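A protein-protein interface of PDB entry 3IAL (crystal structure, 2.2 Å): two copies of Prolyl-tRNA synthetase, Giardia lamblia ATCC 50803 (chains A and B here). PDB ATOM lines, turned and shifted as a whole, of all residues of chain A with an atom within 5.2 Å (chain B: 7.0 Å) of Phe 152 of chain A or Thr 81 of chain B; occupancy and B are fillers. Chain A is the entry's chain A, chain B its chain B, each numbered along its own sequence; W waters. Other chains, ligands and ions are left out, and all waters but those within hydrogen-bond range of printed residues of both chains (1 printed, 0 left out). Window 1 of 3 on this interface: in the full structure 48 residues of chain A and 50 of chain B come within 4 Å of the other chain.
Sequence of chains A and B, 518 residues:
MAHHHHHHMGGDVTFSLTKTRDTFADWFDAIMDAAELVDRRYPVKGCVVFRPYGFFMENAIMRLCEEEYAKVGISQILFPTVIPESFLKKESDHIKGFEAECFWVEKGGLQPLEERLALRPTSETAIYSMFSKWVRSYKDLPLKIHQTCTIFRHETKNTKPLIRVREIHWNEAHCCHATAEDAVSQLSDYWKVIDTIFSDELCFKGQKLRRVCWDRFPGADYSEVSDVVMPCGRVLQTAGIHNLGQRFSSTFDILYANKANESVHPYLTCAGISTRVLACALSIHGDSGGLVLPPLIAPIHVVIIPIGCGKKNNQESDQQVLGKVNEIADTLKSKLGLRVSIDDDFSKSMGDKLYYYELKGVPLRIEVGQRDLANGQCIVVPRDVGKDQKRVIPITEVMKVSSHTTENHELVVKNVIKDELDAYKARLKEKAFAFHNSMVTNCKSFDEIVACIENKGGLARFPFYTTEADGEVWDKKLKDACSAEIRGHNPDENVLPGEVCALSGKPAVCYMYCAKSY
Printed residues of chain A within 4 Å of Pro 80 of chain B: Glu 167. Of the printed residues of chain A, Leu 119 of chain B touches Leu 119. Of the printed residues of chain B, Thr 150 of chain A touches Thr 81 (3.9 Å). Phe 79 of chain B touches none of the printed residues of chain A. Val 82 of chain B touches none of the printed residues of chain A. The nearest residue of chain B that does not touch Phe 152 of chain A is Val 82 of chain B (4.6 Å). The nearest printed residue of chain A that does not touch Thr 81 of chain B is Thr 81 of chain A (5.5 Å).
The side-chain carboxylate (OE2) of Glu 167 of chain A sits at hydrogen-bond distance from the side-chain hydroxyl (OG1) of Thr 81 of chain B, at 2.7 Å.
Printed residues of chain B that touch a printed residue of chain A: Pro 80, Thr 81, Leu 119, Thr 150 and Phe 152. Of the 14 printed residues of chain A, 5 touch a printed residue of chain B. Printed residues of chain A that touch a printed residue of chain B: Thr 81, Leu 119, Thr 150, Phe 152 and Glu 167. Hydrophobic or aromatic side chains of chain A within 4 Å of the printed part of chain B: Leu 119 and Phe 152. Among the printed residues, no Asp or Glu carboxylate lies within 4 Å of a Lys or Arg side-chain nitrogen of the other chain.
The backbone NH (N) of Arg 120 of chain A lies within hydrogen-bond range of the backbone carbonyl oxygen (O) of Thr 81 of chain A, at 3.0 Å. N of Leu 119 of chain A is in hydrogen-bond range of O of Phe 103 of chain A, 3.1 Å away. The guanidinium group of Arg 120 of chain A lies within hydrogen-bond range of the backbone carbonyl oxygen of Thr 150 of chain A. O of Arg 120 of chain A is in hydrogen-bond range of N of Phe 152 of chain A. OE2 of Glu 167 of chain A sits at hydrogen-bond distance from OG1 of Thr 150 of chain A (2.9 Å). The guanidinium group of Arg 120 of chain B sits at hydrogen-bond distance from the backbone carbonyl oxygen of Thr 150 of chain B (3.0 Å).
OG1 of Thr 81 of chain A touches OG1 of Thr 150 of chain B, at 3.96 Å. Phe 152 of chain B touches Thr 81 of chain A. CD2 of Leu 119 of chain B touches CD2 of Leu 119 of chain A (3.8 Å). Thr 81 of chain B touches Thr 150 of chain A. Phe 152 of chain A touches Thr 81 of chain B (CZ to OG1, 3.5 Å). Glu 167 of chain A touches Pro 80 of chain B.
Thr 81 of chain A touches Thr 150 of chain B, and with the chains exchanged Thr 150 of chain A touches Thr 81 of chain B. Thr 81 of chain A touches Phe 152 of chain B, and with the chains exchanged Phe 152 of chain A touches Thr 81 of chain B. Leu 119 of chain A touches its own counterpart, Leu 119 of chain B.
Water W1 lies within hydrogen-bond range of O of Phe 79 of chain B, OE2 of Glu 167 of chain A and NH2 of Arg 120 of chain B.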
ATOM      1  N   THR A  81      22.590  -3.313 -15.764  1.00  0.00           N
ATOM      2  CA  THR A  81      23.414  -3.670 -14.612  1.00  0.00           C
ATOM      3  C   THR A  81      24.063  -5.051 -14.737  1.00  0.00           C
ATOM      4  O   THR A  81      25.169  -5.279 -14.237  1.00  0.00           O
ATOM      5  CB  THR A  81      22.561  -3.680 -13.329  1.00  0.00           C
ATOM      6  OG1 THR A  81      21.902  -2.419 -13.180  1.00  0.00           O
ATOM      7  CG2 THR A  81      23.424  -3.958 -12.096  1.00  0.00           C
ATOM      8  N   GLU A 101      35.774  -9.988  -7.366  1.00  0.00           N
ATOM      9  CA  GLU A 101      34.804  -8.977  -6.938  1.00  0.00           C
ATOM     10  C   GLU A 101      33.421  -9.090  -7.586  1.00  0.00           C
ATOM     11  O   GLU A 101      32.599  -8.205  -7.425  1.00  0.00           O
ATOM     12  CB  GLU A 101      35.407  -7.574  -7.130  1.00  0.00           C
ATOM     13  CG  GLU A 101      36.405  -7.231  -6.010  1.00  0.00           C
ATOM     14  CD  GLU A 101      37.342  -6.097  -6.334  1.00  0.00           C
ATOM     15  OE1 GLU A 101      37.172  -5.450  -7.386  1.00  0.00           O
ATOM     16  OE2 GLU A 101      38.266  -5.853  -5.527  1.00  0.00           O
ATOM     17  N   PHE A 103      29.654 -10.251  -7.905  1.00  0.00           N
ATOM     18  CA  PHE A 103      28.417 -10.864  -7.430  1.00  0.00           C
ATOM     19  C   PHE A 103      27.819 -11.609  -8.612  1.00  0.00           C
ATOM     20  O   PHE A 103      27.725 -11.053  -9.709  1.00  0.00           O
ATOM     21  CB  PHE A 103      27.417  -9.825  -6.947  1.00  0.00           C
ATOM     22  CG  PHE A 103      27.812  -9.124  -5.679  1.00  0.00           C
ATOM     23  CD1 PHE A 103      27.349  -9.570  -4.456  1.00  0.00           C
ATOM     24  CD2 PHE A 103      28.609  -7.994  -5.719  1.00  0.00           C
ATOM     25  CE1 PHE A 103      27.690  -8.906  -3.279  1.00  0.00           C
ATOM     26  CE2 PHE A 103      28.955  -7.324  -4.560  1.00  0.00           C
ATOM     27  CZ  PHE A 103      28.491  -7.777  -3.335  1.00  0.00           C
ATOM     28  N   LEU A 119      26.770  -8.867 -11.710  1.00  0.00           N
ATOM     29  CA  LEU A 119      26.528  -7.458 -11.445  1.00  0.00           C
ATOM     30  C   LEU A 119      27.803  -6.686 -11.810  1.00  0.00           C
ATOM     31  O   LEU A 119      28.908  -7.044 -11.389  1.00  0.00           O
ATOM     32  CB  LEU A 119      26.129  -7.223  -9.982  1.00  0.00           C
ATOM     33  CG  LEU A 119      24.898  -8.006  -9.488  1.00  0.00           C
ATOM     34  CD1 LEU A 119      24.521  -7.646  -8.055  1.00  0.00           C
ATOM     35  CD2 LEU A 119      23.720  -7.777 -10.400  1.00  0.00           C
ATOM     36  N   ARG A 120      27.645  -5.648 -12.624  1.00  0.00           N
ATOM     37  CA  ARG A 120      28.778  -4.911 -13.177  1.00  0.00           C
ATOM     38  C   ARG A 120      29.766  -4.429 -12.101  1.00  0.00           C
ATOM     39  O   ARG A 120      29.383  -3.663 -11.219  1.00  0.00           O
ATOM     40  CB  ARG A 120      28.277  -3.711 -13.993  1.00  0.00           C
ATOM     41  CG  ARG A 120      27.399  -2.736 -13.225  1.00  0.00           C
ATOM     42  CD  ARG A 120      26.913  -1.613 -14.114  1.00  0.00           C
ATOM     43  NE  ARG A 120      25.764  -0.948 -13.513  1.00  0.00           N
ATOM     44  CZ  ARG A 120      24.771  -0.370 -14.190  1.00  0.00           C
ATOM     45  NH1 ARG A 120      24.759  -0.365 -15.523  1.00  0.00           N
ATOM     46  NH2 ARG A 120      23.768   0.193 -13.527  1.00  0.00           N
ATOM     47  N   PRO A 121      31.030  -4.900 -12.155  1.00  0.00           N
ATOM     48  CA  PRO A 121      32.060  -4.330 -11.287  1.00  0.00           C
ATOM     49  C   PRO A 121      32.621  -3.058 -11.892  1.00  0.00           C
ATOM     50  O   PRO A 121      33.190  -2.222 -11.185  1.00  0.00           O
ATOM     51  CB  PRO A 121      33.123  -5.419 -11.253  1.00  0.00           C
ATOM     52  CG  PRO A 121      32.991  -6.091 -12.572  1.00  0.00           C
ATOM     53  CD  PRO A 121      31.551  -6.025 -12.950  1.00  0.00           C
ATOM     54  N   THR A 150      25.314   2.541 -10.347  1.00  0.00           N
ATOM     55  CA  THR A 150      26.105   1.852  -9.342  1.00  0.00           C
ATOM     56  C   THR A 150      26.778   0.614  -9.912  1.00  0.00           C
ATOM     57  O   THR A 150      26.243  -0.074 -10.809  1.00  0.00           O
ATOM     58  CB  THR A 150      25.287   1.443  -8.088  1.00  0.00           C
ATOM     59  OG1 THR A 150      24.328   0.431  -8.428  1.00  0.00           O
ATOM     60  CG2 THR A 150      24.598   2.639  -7.464  1.00  0.00           C
ATOM     61  N   ILE A 151      27.954   0.330  -9.359  1.00  0.00           N
ATOM     62  CA  ILE A 151      28.708  -0.869  -9.680  1.00  0.00           C
ATOM     63  C   ILE A 151      28.888  -1.686  -8.408  1.00  0.00           C
ATOM     64  O   ILE A 151      28.621  -1.199  -7.299  1.00  0.00           O
ATOM     65  CB  ILE A 151      30.082  -0.535 -10.293  1.00  0.00           C
ATOM     66  CG1 ILE A 151      30.862   0.443  -9.397  1.00  0.00           C
ATOM     67  CG2 ILE A 151      29.901   0.034 -11.683  1.00  0.00           C
ATOM     68  CD1 ILE A 151      32.322   0.655  -9.823  1.00  0.00           C
ATOM     69  N   PHE A 152      29.359  -2.916  -8.571  1.00  0.00           N
ATOM     70  CA  PHE A 152      29.382  -3.886  -7.478  1.00  0.00           C
ATOM     71  C   PHE A 152      30.732  -4.584  -7.360  1.00  0.00           C
ATOM     72  O   PHE A 152      31.210  -5.170  -8.324  1.00  0.00           O
ATOM     73  CB  PHE A 152      28.281  -4.923  -7.698  1.00  0.00           C
ATOM     74  CG  PHE A 152      26.899  -4.343  -7.675  1.00  0.00           C
ATOM     75  CD1 PHE A 152      26.146  -4.362  -6.516  1.00  0.00           C
ATOM     76  CD2 PHE A 152      26.359  -3.755  -8.810  1.00  0.00           C
ATOM     77  CE1 PHE A 152      24.880  -3.824  -6.498  1.00  0.00           C
ATOM     78  CE2 PHE A 152      25.104  -3.218  -8.790  1.00  0.00           C
ATOM     79  CZ  PHE A 152      24.359  -3.258  -7.642  1.00  0.00           C
ATOM     80  N   ARG A 153      31.328  -4.522  -6.173  1.00  0.00           N
ATOM     81  CA  ARG A 153      32.641  -5.099  -5.903  1.00  0.00           C
ATOM     82  C   ARG A 153      32.519  -5.905  -4.619  1.00  0.00           C
ATOM     83  O   ARG A 153      32.517  -5.336  -3.525  1.00  0.00           O
ATOM     84  CB  ARG A 153      33.715  -4.004  -5.722  1.00  0.00           C
ATOM     85  CG  ARG A 153      33.831  -2.957  -6.826  1.00  0.00           C
ATOM     86  CD  ARG A 153      34.742  -3.373  -7.951  1.00  0.00           C
ATOM     87  NE  ARG A 153      34.781  -2.385  -9.038  1.00  0.00           N
ATOM     88  CZ  ARG A 153      35.748  -1.489  -9.254  1.00  0.00           C
ATOM     89  NH1 ARG A 153      36.816  -1.401  -8.463  1.00  0.00           N
ATOM     90  NH2 ARG A 153      35.651  -0.663 -10.289  1.00  0.00           N
ATOM     91  N   HIS A 154      32.410  -7.227  -4.754  1.00  0.00           N
ATOM     92  CA  HIS A 154      32.133  -8.109  -3.618  1.00  0.00           C
ATOM     93  C   HIS A 154      33.272  -8.182  -2.614  1.00  0.00           C
ATOM     94  O   HIS A 154      33.032  -8.179  -1.408  1.00  0.00           O
ATOM     95  CB  HIS A 154      31.818  -9.533  -4.091  1.00  0.00           C
ATOM     96  CG  HIS A 154      31.963 -10.563  -3.014  1.00  0.00           C
ATOM     97  ND1 HIS A 154      31.032 -10.722  -2.011  1.00  0.00           N
ATOM     98  CD2 HIS A 154      32.938 -11.467  -2.768  1.00  0.00           C
ATOM     99  CE1 HIS A 154      31.422 -11.685  -1.197  1.00  0.00           C
ATOM    100  NE2 HIS A 154      32.577 -12.154  -1.634  1.00  0.00           N
ATOM    101  N   ARG A 166      30.675  -1.893  -1.242  1.00  0.00           N
ATOM    102  CA  ARG A 166      30.445  -3.041  -2.113  1.00  0.00           C
ATOM    103  C   ARG A 166      29.446  -2.709  -3.212  1.00  0.00           C
ATOM    104  O   ARG A 166      29.535  -3.259  -4.300  1.00  0.00           O
ATOM    105  CB  ARG A 166      30.020  -4.267  -1.294  1.00  0.00           C
ATOM    106  CG  ARG A 166      31.192  -4.882  -0.524  1.00  0.00           C
ATOM    107  CD  ARG A 166      30.782  -5.918   0.498  1.00  0.00           C
ATOM    108  NE  ARG A 166      30.418  -7.202  -0.102  1.00  0.00           N
ATOM    109  CZ  ARG A 166      29.286  -7.882   0.120  1.00  0.00           C
ATOM    110  NH1 ARG A 166      28.341  -7.440   0.941  1.00  0.00           N
ATOM    111  NH2 ARG A 166      29.101  -9.042  -0.494  1.00  0.00           N
ATOM    112  N   GLU A 167      28.501  -1.816  -2.937  1.00  0.00           N
ATOM    113  CA  GLU A 167      27.743  -1.159  -4.005  1.00  0.00           C
ATOM    114  C   GLU A 167      28.119   0.315  -4.037  1.00  0.00           C
ATOM    115  O   GLU A 167      27.902   1.042  -3.076  1.00  0.00           O
ATOM    116  CB  GLU A 167      26.228  -1.303  -3.833  1.00  0.00           C
ATOM    117  CG  GLU A 167      25.457  -0.635  -4.985  1.00  0.00           C
ATOM    118  CD  GLU A 167      23.967  -0.912  -4.971  1.00  0.00           C
ATOM    119  OE1 GLU A 167      23.499  -1.671  -4.094  1.00  0.00           O
ATOM    120  OE2 GLU A 167      23.264  -0.378  -5.857  1.00  0.00           O
ATOM    121  N   ILE A 168      28.637   0.742  -5.182  1.00  0.00           N
ATOM    122  CA  ILE A 168      29.330   1.994  -5.317  1.00  0.00           C
ATOM    123  C   ILE A 168      28.616   2.891  -6.309  1.00  0.00           C
ATOM    124  O   ILE A 168      28.462   2.517  -7.459  1.00  0.00           O
ATOM    125  CB  ILE A 168      30.743   1.742  -5.864  1.00  0.00           C
ATOM    126  CG1 ILE A 168      31.436   0.639  -5.047  1.00  0.00           C
ATOM    127  CG2 ILE A 168      31.537   3.044  -5.890  1.00  0.00           C
ATOM    128  CD1 ILE A 168      32.547  -0.045  -5.781  1.00  0.00           C
ATOM    129  N   LEU B  78      18.663   7.225  -2.162  1.00  0.00           N
ATOM    130  CA  LEU B  78      18.993   6.011  -2.915  1.00  0.00           C
ATOM    131  C   LEU B  78      19.302   4.833  -1.994  1.00  0.00           C
ATOM    132  O   LEU B  78      20.165   4.930  -1.104  1.00  0.00           O
ATOM    133  CB  LEU B  78      20.167   6.244  -3.870  1.00  0.00           C
ATOM    134  CG  LEU B  78      20.526   5.062  -4.796  1.00  0.00           C
ATOM    135  CD1 LEU B  78      19.345   4.716  -5.695  1.00  0.00           C
ATOM    136  CD2 LEU B  78      21.746   5.371  -5.645  1.00  0.00           C
ATOM    137  N   PHE B  79      18.588   3.732  -2.237  1.00  0.00           N
ATOM    138  CA  PHE B  79      18.791   2.469  -1.559  1.00  0.00           C
ATOM    139  C   PHE B  79      19.686   1.583  -2.419  1.00  0.00           C
ATOM    140  O   PHE B  79      19.772   1.793  -3.629  1.00  0.00           O
ATOM    141  CB  PHE B  79      17.448   1.756  -1.322  1.00  0.00           C
ATOM    142  CG  PHE B  79      16.840   2.034   0.024  1.00  0.00           C
ATOM    143  CD1 PHE B  79      16.360   3.293   0.337  1.00  0.00           C
ATOM    144  CD2 PHE B  79      16.763   1.034   0.981  1.00  0.00           C
ATOM    145  CE1 PHE B  79      15.809   3.556   1.584  1.00  0.00           C
ATOM    146  CE2 PHE B  79      16.209   1.285   2.218  1.00  0.00           C
ATOM    147  CZ  PHE B  79      15.733   2.553   2.524  1.00  0.00           C
ATOM    148  N   PRO B  80      20.348   0.580  -1.794  1.00  0.00           N
ATOM    149  CA  PRO B  80      21.051  -0.475  -2.516  1.00  0.00           C
ATOM    150  C   PRO B  80      20.133  -1.282  -3.423  1.00  0.00           C
ATOM    151  O   PRO B  80      18.926  -1.351  -3.192  1.00  0.00           O
ATOM    152  CB  PRO B  80      21.573  -1.380  -1.400  1.00  0.00           C
ATOM    153  CG  PRO B  80      21.671  -0.513  -0.221  1.00  0.00           C
ATOM    154  CD  PRO B  80      20.525   0.436  -0.338  1.00  0.00           C
ATOM    155  N   THR B  81      20.723  -1.886  -4.445  1.00  0.00           N
ATOM    156  CA  THR B  81      19.997  -2.697  -5.412  1.00  0.00           C
ATOM    157  C   THR B  81      19.627  -4.049  -4.823  1.00  0.00           C
ATOM    158  O   THR B  81      18.633  -4.664  -5.220  1.00  0.00           O
ATOM    159  CB  THR B  81      20.870  -2.929  -6.661  1.00  0.00           C
ATOM    160  OG1 THR B  81      21.261  -1.663  -7.197  1.00  0.00           O
ATOM    161  CG2 THR B  81      20.135  -3.743  -7.728  1.00  0.00           C
ATOM    162  N   VAL B  82      20.437  -4.516  -3.888  1.00  0.00           N
ATOM    163  CA  VAL B  82      20.291  -5.867  -3.354  1.00  0.00           C
ATOM    164  C   VAL B  82      19.429  -5.853  -2.094  1.00  0.00           C
ATOM    165  O   VAL B  82      19.590  -4.984  -1.234  1.00  0.00           O
ATOM    166  CB  VAL B  82      21.667  -6.512  -3.073  1.00  0.00           C
ATOM    167  CG1 VAL B  82      22.292  -7.022  -4.384  1.00  0.00           C
ATOM    168  CG2 VAL B  82      22.616  -5.525  -2.355  1.00  0.00           C
ATOM    169  N   ILE B  83      18.499  -6.803  -2.013  1.00  0.00           N
ATOM    170  CA  ILE B  83      17.625  -6.948  -0.860  1.00  0.00           C
ATOM    171  C   ILE B  83      17.866  -8.325  -0.260  1.00  0.00           C
ATOM    172  O   ILE B  83      17.768  -9.320  -0.969  1.00  0.00           O
ATOM    173  CB  ILE B  83      16.128  -6.824  -1.235  1.00  0.00           C
ATOM    174  CG1 ILE B  83      15.843  -5.502  -1.951  1.00  0.00           C
ATOM    175  CG2 ILE B  83      15.251  -6.898   0.014  1.00  0.00           C
ATOM    176  CD1 ILE B  83      14.389  -5.313  -2.328  1.00  0.00           C
ATOM    177  N   LEU B 117      20.806 -12.700  -1.868  1.00  0.00           N
ATOM    178  CA  LEU B 117      20.368 -11.328  -2.127  1.00  0.00           C
ATOM    179  C   LEU B 117      19.527 -11.260  -3.380  1.00  0.00           C
ATOM    180  O   LEU B 117      19.950 -11.712  -4.443  1.00  0.00           O
ATOM    181  CB  LEU B 117      21.572 -10.401  -2.296  1.00  0.00           C
ATOM    182  CG  LEU B 117      22.548 -10.306  -1.119  1.00  0.00           C
ATOM    183  CD1 LEU B 117      23.689  -9.393  -1.502  1.00  0.00           C
ATOM    184  CD2 LEU B 117      21.842  -9.812   0.126  1.00  0.00           C
ATOM    185  N   ALA B 118      18.332 -10.691  -3.262  1.00  0.00           N
ATOM    186  CA  ALA B 118      17.480 -10.479  -4.423  1.00  0.00           C
ATOM    187  C   ALA B 118      17.790  -9.122  -5.039  1.00  0.00           C
ATOM    188  O   ALA B 118      18.011  -8.144  -4.327  1.00  0.00           O
ATOM    189  CB  ALA B 118      16.017 -10.561  -4.033  1.00  0.00           C
ATOM    190  N   LEU B 119      17.830  -9.062  -6.365  1.00  0.00           N
ATOM    191  CA  LEU B 119      17.831  -7.777  -7.041  1.00  0.00           C
ATOM    192  C   LEU B 119      16.413  -7.223  -6.889  1.00  0.00           C
ATOM    193  O   LEU B 119      15.445  -7.932  -7.158  1.00  0.00           O
ATOM    194  CB  LEU B 119      18.186  -7.931  -8.516  1.00  0.00           C
ATOM    195  CG  LEU B 119      19.526  -8.591  -8.856  1.00  0.00           C
ATOM    196  CD1 LEU B 119      19.756  -8.501 -10.355  1.00  0.00           C
ATOM    197  CD2 LEU B 119      20.682  -7.951  -8.090  1.00  0.00           C
ATOM    198  N   ARG B 120      16.295  -5.980  -6.434  1.00  0.00           N
ATOM    199  CA  ARG B 120      14.991  -5.372  -6.157  1.00  0.00           C
ATOM    200  C   ARG B 120      14.007  -5.445  -7.337  1.00  0.00           C
ATOM    201  O   ARG B 120      14.299  -4.954  -8.418  1.00  0.00           O
ATOM    202  CB  ARG B 120      15.156  -3.913  -5.711  1.00  0.00           C
ATOM    203  CG  ARG B 120      15.909  -3.036  -6.684  1.00  0.00           C
ATOM    204  CD  ARG B 120      16.054  -1.631  -6.133  1.00  0.00           C
ATOM    205  NE  ARG B 120      17.012  -0.901  -6.948  1.00  0.00           N
ATOM    206  CZ  ARG B 120      17.845   0.035  -6.512  1.00  0.00           C
ATOM    207  NH1 ARG B 120      17.873   0.420  -5.240  1.00  0.00           N
ATOM    208  NH2 ARG B 120      18.679   0.580  -7.379  1.00  0.00           N
ATOM    209  N   PRO B 121      12.856  -6.100  -7.144  1.00  0.00           N
ATOM    210  CA  PRO B 121      11.771  -5.980  -8.130  1.00  0.00           C
ATOM    211  C   PRO B 121      10.917  -4.740  -7.894  1.00  0.00           C
ATOM    212  O   PRO B 121      10.194  -4.290  -8.778  1.00  0.00           O
ATOM    213  CB  PRO B 121      10.948  -7.237  -7.881  1.00  0.00           C
ATOM    214  CG  PRO B 121      11.133  -7.523  -6.432  1.00  0.00           C
ATOM    215  CD  PRO B 121      12.575  -7.152  -6.149  1.00  0.00           C
ATOM    216  N   SER B 123      10.807  -1.832  -4.133  1.00  0.00           N
ATOM    217  CA  SER B 123      11.623  -1.672  -2.933  1.00  0.00           C
ATOM    218  C   SER B 123      10.902  -1.618  -1.578  1.00  0.00           C
ATOM    219  O   SER B 123      11.542  -1.358  -0.564  1.00  0.00           O
ATOM    220  CB  SER B 123      12.548  -0.463  -3.101  1.00  0.00           C
ATOM    221  OG  SER B 123      13.230  -0.540  -4.343  1.00  0.00           O
ATOM    222  N   CYS B 149      15.875   4.865 -10.097  1.00  0.00           N
ATOM    223  CA  CYS B 149      16.795   3.734 -10.156  1.00  0.00           C
ATOM    224  C   CYS B 149      16.227   2.707 -11.120  1.00  0.00           C
ATOM    225  O   CYS B 149      15.218   2.960 -11.778  1.00  0.00           O
ATOM    226  CB  CYS B 149      16.972   3.106  -8.765  1.00  0.00           C
ATOM    227  SG  CYS B 149      15.470   2.271  -8.114  1.00  0.00           S
ATOM    228  N   THR B 150      16.867   1.546 -11.194  1.00  0.00           N
ATOM    229  CA  THR B 150      16.316   0.443 -11.958  1.00  0.00           C
ATOM    230  C   THR B 150      15.860  -0.648 -10.998  1.00  0.00           C
ATOM    231  O   THR B 150      16.420  -0.800  -9.897  1.00  0.00           O
ATOM    232  CB  THR B 150      17.298  -0.085 -13.027  1.00  0.00           C
ATOM    233  OG1 THR B 150      18.337  -0.873 -12.429  1.00  0.00           O
ATOM    234  CG2 THR B 150      17.908   1.070 -13.799  1.00  0.00           C
ATOM    235  N   ILE B 151      14.807  -1.356 -11.405  1.00  0.00           N
ATOM    236  CA  ILE B 151      14.325  -2.552 -10.718  1.00  0.00           C
ATOM    237  C   ILE B 151      14.429  -3.719 -11.698  1.00  0.00           C
ATOM    238  O   ILE B 151      14.701  -3.506 -12.892  1.00  0.00           O
ATOM    239  CB  ILE B 151      12.871  -2.391 -10.213  1.00  0.00           C
ATOM    240  CG1 ILE B 151      11.947  -1.885 -11.331  1.00  0.00           C
ATOM    241  CG2 ILE B 151      12.831  -1.447  -9.004  1.00  0.00           C
ATOM    242  CD1 ILE B 151      10.456  -2.171 -11.072  1.00  0.00           C
ATOM    243  N   PHE B 152      14.215  -4.938 -11.199  1.00  0.00           N
ATOM    244  CA  PHE B 152      14.473  -6.160 -11.973  1.00  0.00           C
ATOM    245  C   PHE B 152      13.310  -7.157 -11.889  1.00  0.00           C
ATOM    246  O   PHE B 152      12.873  -7.506 -10.798  1.00  0.00           O
ATOM    247  CB  PHE B 152      15.768  -6.823 -11.485  1.00  0.00           C
ATOM    248  CG  PHE B 152      16.989  -5.945 -11.623  1.00  0.00           C
ATOM    249  CD1 PHE B 152      17.827  -6.064 -12.728  1.00  0.00           C
ATOM    250  CD2 PHE B 152      17.298  -5.004 -10.652  1.00  0.00           C
ATOM    251  CE1 PHE B 152      18.949  -5.261 -12.861  1.00  0.00           C
ATOM    252  CE2 PHE B 152      18.430  -4.184 -10.777  1.00  0.00           C
ATOM    253  CZ  PHE B 152      19.252  -4.312 -11.880  1.00  0.00           C
HETATM  254  O   HOH W   1      21.235   1.688  -5.914  1.00  0.00           O
